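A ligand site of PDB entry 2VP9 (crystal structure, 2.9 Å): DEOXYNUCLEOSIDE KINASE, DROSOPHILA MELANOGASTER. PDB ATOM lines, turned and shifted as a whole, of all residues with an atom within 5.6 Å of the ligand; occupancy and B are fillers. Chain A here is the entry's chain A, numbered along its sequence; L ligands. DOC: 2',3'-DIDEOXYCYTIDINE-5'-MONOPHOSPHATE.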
ATOM      1  N   ILE A  29      22.342  14.776  21.120  1.00  0.00           N
ATOM      2  CA  ILE A  29      23.740  14.556  21.017  1.00  0.00           C
ATOM      3  C   ILE A  29      24.281  15.408  22.134  1.00  0.00           C
ATOM      4  O   ILE A  29      23.824  16.525  22.349  1.00  0.00           O
ATOM      5  CB  ILE A  29      24.295  15.046  19.666  1.00  0.00           C
ATOM      6  CG1 ILE A  29      23.444  14.532  18.497  1.00  0.00           C
ATOM      7  CG2 ILE A  29      25.750  14.627  19.498  1.00  0.00           C
ATOM      8  CD1 ILE A  29      23.831  15.080  17.141  1.00  0.00           C
ATOM      9  N   LYS A  33      24.520  10.705  27.569  1.00  0.00           N
ATOM     10  CA  LYS A  33      24.045   9.342  27.545  1.00  0.00           C
ATOM     11  C   LYS A  33      25.173   8.368  27.811  1.00  0.00           C
ATOM     12  O   LYS A  33      25.025   7.496  28.647  1.00  0.00           O
ATOM     13  CB  LYS A  33      23.320   9.046  26.243  1.00  0.00           C
ATOM     14  CG  LYS A  33      21.946   9.670  26.150  1.00  0.00           C
ATOM     15  CD  LYS A  33      21.287   9.400  24.834  1.00  0.00           C
ATOM     16  CE  LYS A  33      21.821  10.287  23.720  1.00  0.00           C
ATOM     17  NZ  LYS A  33      22.959   9.703  22.969  1.00  0.00           N
ATOM     18  N   GLU A  52      24.696   2.622  21.897  1.00  0.00           N
ATOM     19  CA  GLU A  52      24.429   2.941  20.499  1.00  0.00           C
ATOM     20  C   GLU A  52      25.515   2.333  19.617  1.00  0.00           C
ATOM     21  O   GLU A  52      26.690   2.494  19.936  1.00  0.00           O
ATOM     22  CB  GLU A  52      24.374   4.456  20.334  1.00  0.00           C
ATOM     23  CG  GLU A  52      23.445   4.938  19.263  1.00  0.00           C
ATOM     24  CD  GLU A  52      23.562   6.417  19.022  1.00  0.00           C
ATOM     25  OE1 GLU A  52      24.646   6.967  19.179  1.00  0.00           O
ATOM     26  OE2 GLU A  52      22.557   7.061  18.675  1.00  0.00           O
ATOM     27  N   VAL A  54      27.498   2.835  17.219  1.00  0.00           N
ATOM     28  CA  VAL A  54      28.248   3.770  16.420  1.00  0.00           C
ATOM     29  C   VAL A  54      29.389   3.029  15.690  1.00  0.00           C
ATOM     30  O   VAL A  54      29.690   3.333  14.549  1.00  0.00           O
ATOM     31  CB  VAL A  54      28.815   4.898  17.303  1.00  0.00           C
ATOM     32  CG1 VAL A  54      29.080   6.113  16.489  1.00  0.00           C
ATOM     33  CG2 VAL A  54      27.867   5.248  18.416  1.00  0.00           C
ATOM     34  N   TRP A  57      28.376   1.619  12.494  1.00  0.00           N
ATOM     35  CA  TRP A  57      28.140   2.627  11.468  1.00  0.00           C
ATOM     36  C   TRP A  57      29.460   3.149  10.883  1.00  0.00           C
ATOM     37  O   TRP A  57      29.479   3.730   9.789  1.00  0.00           O
ATOM     38  CB  TRP A  57      27.311   3.813  11.981  1.00  0.00           C
ATOM     39  CG  TRP A  57      26.090   3.481  12.752  1.00  0.00           C
ATOM     40  CD1 TRP A  57      25.349   2.375  12.662  1.00  0.00           C
ATOM     41  CD2 TRP A  57      25.469   4.293  13.737  1.00  0.00           C
ATOM     42  NE1 TRP A  57      24.307   2.417  13.529  1.00  0.00           N
ATOM     43  CE2 TRP A  57      24.355   3.598  14.211  1.00  0.00           C
ATOM     44  CE3 TRP A  57      25.745   5.559  14.267  1.00  0.00           C
ATOM     45  CZ2 TRP A  57      23.526   4.100  15.181  1.00  0.00           C
ATOM     46  CZ3 TRP A  57      24.916   6.067  15.244  1.00  0.00           C
ATOM     47  CH2 TRP A  57      23.815   5.332  15.685  1.00  0.00           C
ATOM     48  N   LEU A  66      28.848   7.063   8.931  1.00  0.00           N
ATOM     49  CA  LEU A  66      28.680   8.221   9.792  1.00  0.00           C
ATOM     50  C   LEU A  66      29.417   9.443   9.239  1.00  0.00           C
ATOM     51  O   LEU A  66      28.841  10.520   9.188  1.00  0.00           O
ATOM     52  CB  LEU A  66      29.119   7.915  11.227  1.00  0.00           C
ATOM     53  CG  LEU A  66      28.858   8.985  12.295  1.00  0.00           C
ATOM     54  CD1 LEU A  66      27.420   9.424  12.305  1.00  0.00           C
ATOM     55  CD2 LEU A  66      29.257   8.491  13.654  1.00  0.00           C
ATOM     56  N   MET A  69      28.011  10.656   5.910  1.00  0.00           N
ATOM     57  CA  MET A  69      26.781  11.344   6.189  1.00  0.00           C
ATOM     58  C   MET A  69      27.034  12.790   6.616  1.00  0.00           C
ATOM     59  O   MET A  69      26.341  13.697   6.185  1.00  0.00           O
ATOM     60  CB  MET A  69      25.976  10.591   7.233  1.00  0.00           C
ATOM     61  CG  MET A  69      24.634  11.213   7.563  1.00  0.00           C
ATOM     62  SD  MET A  69      24.728  12.543   8.801  1.00  0.00           S
ATOM     63  CE  MET A  69      25.085  11.639  10.298  1.00  0.00           C
ATOM     64  N   TYR A  70      28.036  13.004   7.459  1.00  0.00           N
ATOM     65  CA  TYR A  70      28.361  14.373   7.902  1.00  0.00           C
ATOM     66  C   TYR A  70      29.112  15.193   6.847  1.00  0.00           C
ATOM     67  O   TYR A  70      29.134  16.424   6.915  1.00  0.00           O
ATOM     68  CB  TYR A  70      29.136  14.373   9.217  1.00  0.00           C
ATOM     69  CG  TYR A  70      28.258  14.265  10.446  1.00  0.00           C
ATOM     70  CD1 TYR A  70      28.530  13.331  11.449  1.00  0.00           C
ATOM     71  CD2 TYR A  70      27.151  15.106  10.605  1.00  0.00           C
ATOM     72  CE1 TYR A  70      27.726  13.235  12.584  1.00  0.00           C
ATOM     73  CE2 TYR A  70      26.350  15.028  11.727  1.00  0.00           C
ATOM     74  CZ  TYR A  70      26.620  14.081  12.714  1.00  0.00           C
ATOM     75  OH  TYR A  70      25.813  13.990  13.833  1.00  0.00           O
ATOM     76  N   PHE A  80      22.741   6.040   5.266  1.00  0.00           N
ATOM     77  CA  PHE A  80      23.106   6.085   6.672  1.00  0.00           C
ATOM     78  C   PHE A  80      21.943   5.728   7.613  1.00  0.00           C
ATOM     79  O   PHE A  80      22.076   4.868   8.479  1.00  0.00           O
ATOM     80  CB  PHE A  80      23.718   7.445   7.020  1.00  0.00           C
ATOM     81  CG  PHE A  80      23.915   7.632   8.482  1.00  0.00           C
ATOM     82  CD1 PHE A  80      24.949   6.980   9.153  1.00  0.00           C
ATOM     83  CD2 PHE A  80      23.021   8.402   9.230  1.00  0.00           C
ATOM     84  CE1 PHE A  80      25.125   7.137  10.525  1.00  0.00           C
ATOM     85  CE2 PHE A  80      23.195   8.547  10.587  1.00  0.00           C
ATOM     86  CZ  PHE A  80      24.244   7.908  11.233  1.00  0.00           C
ATOM     87  N   GLN A  81      20.801   6.406   7.443  1.00  0.00           N
ATOM     88  CA  GLN A  81      19.663   6.213   8.327  1.00  0.00           C
ATOM     89  C   GLN A  81      19.073   4.828   8.151  1.00  0.00           C
ATOM     90  O   GLN A  81      18.666   4.164   9.140  1.00  0.00           O
ATOM     91  CB  GLN A  81      18.620   7.299   8.092  1.00  0.00           C
ATOM     92  CG  GLN A  81      19.064   8.653   8.614  1.00  0.00           C
ATOM     93  CD  GLN A  81      19.310   8.686  10.143  1.00  0.00           C
ATOM     94  OE1 GLN A  81      19.982   9.582  10.663  1.00  0.00           O
ATOM     95  NE2 GLN A  81      18.746   7.717  10.864  1.00  0.00           N
ATOM     96  N   VAL A  84      21.273   2.765  10.240  1.00  0.00           N
ATOM     97  CA  VAL A  84      20.975   2.991  11.652  1.00  0.00           C
ATOM     98  C   VAL A  84      19.732   2.191  11.990  1.00  0.00           C
ATOM     99  O   VAL A  84      19.780   1.337  12.872  1.00  0.00           O
ATOM    100  CB  VAL A  84      20.791   4.505  11.973  1.00  0.00           C
ATOM    101  CG1 VAL A  84      20.322   4.735  13.370  1.00  0.00           C
ATOM    102  CG2 VAL A  84      22.060   5.259  11.733  1.00  0.00           C
ATOM    103  N   MET A  88      19.488  -0.660  14.901  1.00  0.00           N
ATOM    104  CA  MET A  88      18.609  -0.481  16.029  1.00  0.00           C
ATOM    105  C   MET A  88      17.693  -1.644  16.154  1.00  0.00           C
ATOM    106  O   MET A  88      17.465  -2.127  17.251  1.00  0.00           O
ATOM    107  CB  MET A  88      17.840   0.825  15.928  1.00  0.00           C
ATOM    108  CG  MET A  88      18.727   2.061  16.145  1.00  0.00           C
ATOM    109  SD  MET A  88      19.931   1.926  17.518  1.00  0.00           S
ATOM    110  CE  MET A  88      20.623   3.540  17.335  1.00  0.00           C
ATOM    111  N   ARG A 105      19.198   5.013  22.891  1.00  0.00           N
ATOM    112  CA  ARG A 105      18.406   5.400  21.717  1.00  0.00           C
ATOM    113  C   ARG A 105      17.613   4.211  21.159  1.00  0.00           C
ATOM    114  O   ARG A 105      17.648   3.116  21.696  1.00  0.00           O
ATOM    115  CB  ARG A 105      19.295   6.052  20.618  1.00  0.00           C
ATOM    116  CG  ARG A 105      19.950   7.389  20.980  1.00  0.00           C
ATOM    117  CD  ARG A 105      20.030   8.278  19.777  1.00  0.00           C
ATOM    118  NE  ARG A 105      20.267   9.666  20.123  1.00  0.00           N
ATOM    119  CZ  ARG A 105      21.447  10.251  20.052  1.00  0.00           C
ATOM    120  NH1 ARG A 105      22.496   9.557  19.665  1.00  0.00           N
ATOM    121  NH2 ARG A 105      21.608  11.529  20.377  1.00  0.00           N
ATOM    122  N   SER A 109      13.765   7.188  18.077  1.00  0.00           N
ATOM    123  CA  SER A 109      14.502   8.433  17.980  1.00  0.00           C
ATOM    124  C   SER A 109      15.016   8.611  16.574  1.00  0.00           C
ATOM    125  O   SER A 109      15.095   9.719  16.069  1.00  0.00           O
ATOM    126  CB  SER A 109      15.638   8.461  18.972  1.00  0.00           C
ATOM    127  OG  SER A 109      16.163   7.155  19.197  1.00  0.00           O
ATOM    128  N   ALA A 110      15.347   7.514  15.919  1.00  0.00           N
ATOM    129  CA  ALA A 110      15.782   7.566  14.544  1.00  0.00           C
ATOM    130  C   ALA A 110      14.662   8.121  13.625  1.00  0.00           C
ATOM    131  O   ALA A 110      14.875   9.055  12.835  1.00  0.00           O
ATOM    132  CB  ALA A 110      16.211   6.210  14.100  1.00  0.00           C
ATOM    133  N   PHE A 114      16.002  12.236  14.236  1.00  0.00           N
ATOM    134  CA  PHE A 114      17.065  12.399  13.281  1.00  0.00           C
ATOM    135  C   PHE A 114      16.570  12.392  11.830  1.00  0.00           C
ATOM    136  O   PHE A 114      16.938  13.261  11.040  1.00  0.00           O
ATOM    137  CB  PHE A 114      18.206  11.379  13.543  1.00  0.00           C
ATOM    138  CG  PHE A 114      18.828  11.541  14.897  1.00  0.00           C
ATOM    139  CD1 PHE A 114      18.256  10.934  16.009  1.00  0.00           C
ATOM    140  CD2 PHE A 114      19.920  12.344  15.083  1.00  0.00           C
ATOM    141  CE1 PHE A 114      18.794  11.098  17.267  1.00  0.00           C
ATOM    142  CE2 PHE A 114      20.434  12.533  16.347  1.00  0.00           C
ATOM    143  CZ  PHE A 114      19.859  11.908  17.436  1.00  0.00           C
ATOM    144  N   VAL A 115      15.719  11.441  11.472  1.00  0.00           N
ATOM    145  CA  VAL A 115      15.260  11.408  10.116  1.00  0.00           C
ATOM    146  C   VAL A 115      14.391  12.623   9.853  1.00  0.00           C
ATOM    147  O   VAL A 115      14.559  13.316   8.849  1.00  0.00           O
ATOM    148  CB  VAL A 115      14.548  10.081   9.764  1.00  0.00           C
ATOM    149  CG1 VAL A 115      13.625  10.232   8.534  1.00  0.00           C
ATOM    150  CG2 VAL A 115      15.598   8.991   9.552  1.00  0.00           C
ATOM    151  N   MET A 118      16.503  15.629   9.191  1.00  0.00           N
ATOM    152  CA  MET A 118      17.132  15.617   7.874  1.00  0.00           C
ATOM    153  C   MET A 118      16.204  15.916   6.719  1.00  0.00           C
ATOM    154  O   MET A 118      16.614  16.528   5.746  1.00  0.00           O
ATOM    155  CB  MET A 118      17.853  14.299   7.643  1.00  0.00           C
ATOM    156  CG  MET A 118      19.268  14.403   8.037  1.00  0.00           C
ATOM    157  SD  MET A 118      19.929  12.785   7.998  1.00  0.00           S
ATOM    158  CE  MET A 118      21.651  13.154   7.730  1.00  0.00           C
ATOM    159  N   GLU A 172      30.262  14.374  14.911  1.00  0.00           N
ATOM    160  CA  GLU A 172      29.274  15.325  15.382  1.00  0.00           C
ATOM    161  C   GLU A 172      29.831  16.677  15.883  1.00  0.00           C
ATOM    162  O   GLU A 172      29.086  17.614  16.138  1.00  0.00           O
ATOM    163  CB  GLU A 172      28.495  14.643  16.496  1.00  0.00           C
ATOM    164  CG  GLU A 172      29.239  13.422  17.083  1.00  0.00           C
ATOM    165  CD  GLU A 172      29.029  13.260  18.564  1.00  0.00           C
ATOM    166  OE1 GLU A 172      29.051  14.264  19.287  1.00  0.00           O
ATOM    167  OE2 GLU A 172      28.836  12.141  19.038  1.00  0.00           O
ATOM    168  N   TYR A 179      21.524  23.235  14.715  1.00  0.00           N
ATOM    169  CA  TYR A 179      21.181  21.843  14.498  1.00  0.00           C
ATOM    170  C   TYR A 179      20.787  21.200  15.828  1.00  0.00           C
ATOM    171  O   TYR A 179      19.759  20.526  15.906  1.00  0.00           O
ATOM    172  CB  TYR A 179      22.377  21.154  13.863  1.00  0.00           C
ATOM    173  CG  TYR A 179      22.273  19.681  13.547  1.00  0.00           C
ATOM    174  CD1 TYR A 179      21.532  19.221  12.454  1.00  0.00           C
ATOM    175  CD2 TYR A 179      22.976  18.758  14.310  1.00  0.00           C
ATOM    176  CE1 TYR A 179      21.461  17.834  12.143  1.00  0.00           C
ATOM    177  CE2 TYR A 179      22.935  17.394  14.017  1.00  0.00           C
ATOM    178  CZ  TYR A 179      22.184  16.933  12.951  1.00  0.00           C
ATOM    179  OH  TYR A 179      22.197  15.579  12.722  1.00  0.00           O
HETATM  180  N1  DOC L   1      22.841   9.919  14.678  1.00  0.00           N
HETATM  181  C2  DOC L   1      22.055  10.244  13.528  1.00  0.00           C
HETATM  182  N3  DOC L   1      20.877   9.614  13.315  1.00  0.00           N
HETATM  183  C4  DOC L   1      20.431   8.660  14.167  1.00  0.00           C
HETATM  184  C5  DOC L   1      21.196   8.343  15.288  1.00  0.00           C
HETATM  185  C6  DOC L   1      22.394   8.988  15.537  1.00  0.00           C
HETATM  186  O2  DOC L   1      22.427  11.107  12.717  1.00  0.00           O
HETATM  187  N4  DOC L   1      19.235   8.033  13.940  1.00  0.00           N
HETATM  188  C1' DOC L   1      24.096  10.590  14.941  1.00  0.00           C
HETATM  189  C2' DOC L   1      23.869  11.568  16.079  1.00  0.00           C
HETATM  190  C3' DOC L   1      25.271  11.759  16.648  1.00  0.00           C
HETATM  191  C4' DOC L   1      25.997  10.482  16.255  1.00  0.00           C
HETATM  192  O4' DOC L   1      25.126   9.709  15.398  1.00  0.00           O
HETATM  193  C5' DOC L   1      26.341   9.671  17.486  1.00  0.00           C
HETATM  194  O5' DOC L   1      25.186   9.556  18.335  1.00  0.00           O
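The side-chain amide oxygen of Gln 81 sits close to a nitrogen (N3) of the ligand, 2.8 Å away.
The guanidinium group (NH1) of Arg 105 lies within hydrogen-bond range of an oxygen (O5') of the ligand (3.0 Å).
N of Val 115 is in hydrogen-bond range of O of Ala 110 (2.9 Å).
O of Trp 57 sits at hydrogen-bond distance from N of Leu 66 (3.5 Å).
The backbone carbonyl oxygen (O) of Ser 109 lies within hydrogen-bond range of the backbone NH (N) of Phe 114.
OE2 of Glu 52 lies within salt-bridge range of NH1 of Arg 105, at 2.7 Å.
OE1 of Glu 52 sits close to O5' of the ligand (2.8 Å).
CD1 of Ile 29 touches C3' of the ligand, 3.7 Å away.
Trp 57 touches the ligand (CZ3 to O4', 3.7 Å).
CD1 of Leu 66 touches O4' of the ligand, 3.9 Å away.
Met 69 touches the ligand.
OH of Tyr 70 touches C3' of the ligand (3.6 Å).
Phe 80 touches the ligand.
Val 84 touches the ligand.
CB of Ala 110 touches N4 of the ligand, 3.5 Å away.
Phe 114 touches the ligand.
Glu 172 touches the ligand (OE2 to C5', 3.8 Å).
Within 4 Å of the ligand: Ile 29, Glu 52, Trp 57, Leu 66, Met 69, Tyr 70, Phe 80, Gln 81, Val 84, Arg 105, Ala 110, Phe 114 and Glu 172.
The nearest printed residue that does not touch the ligand is Tyr 179 (4.5 Å).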
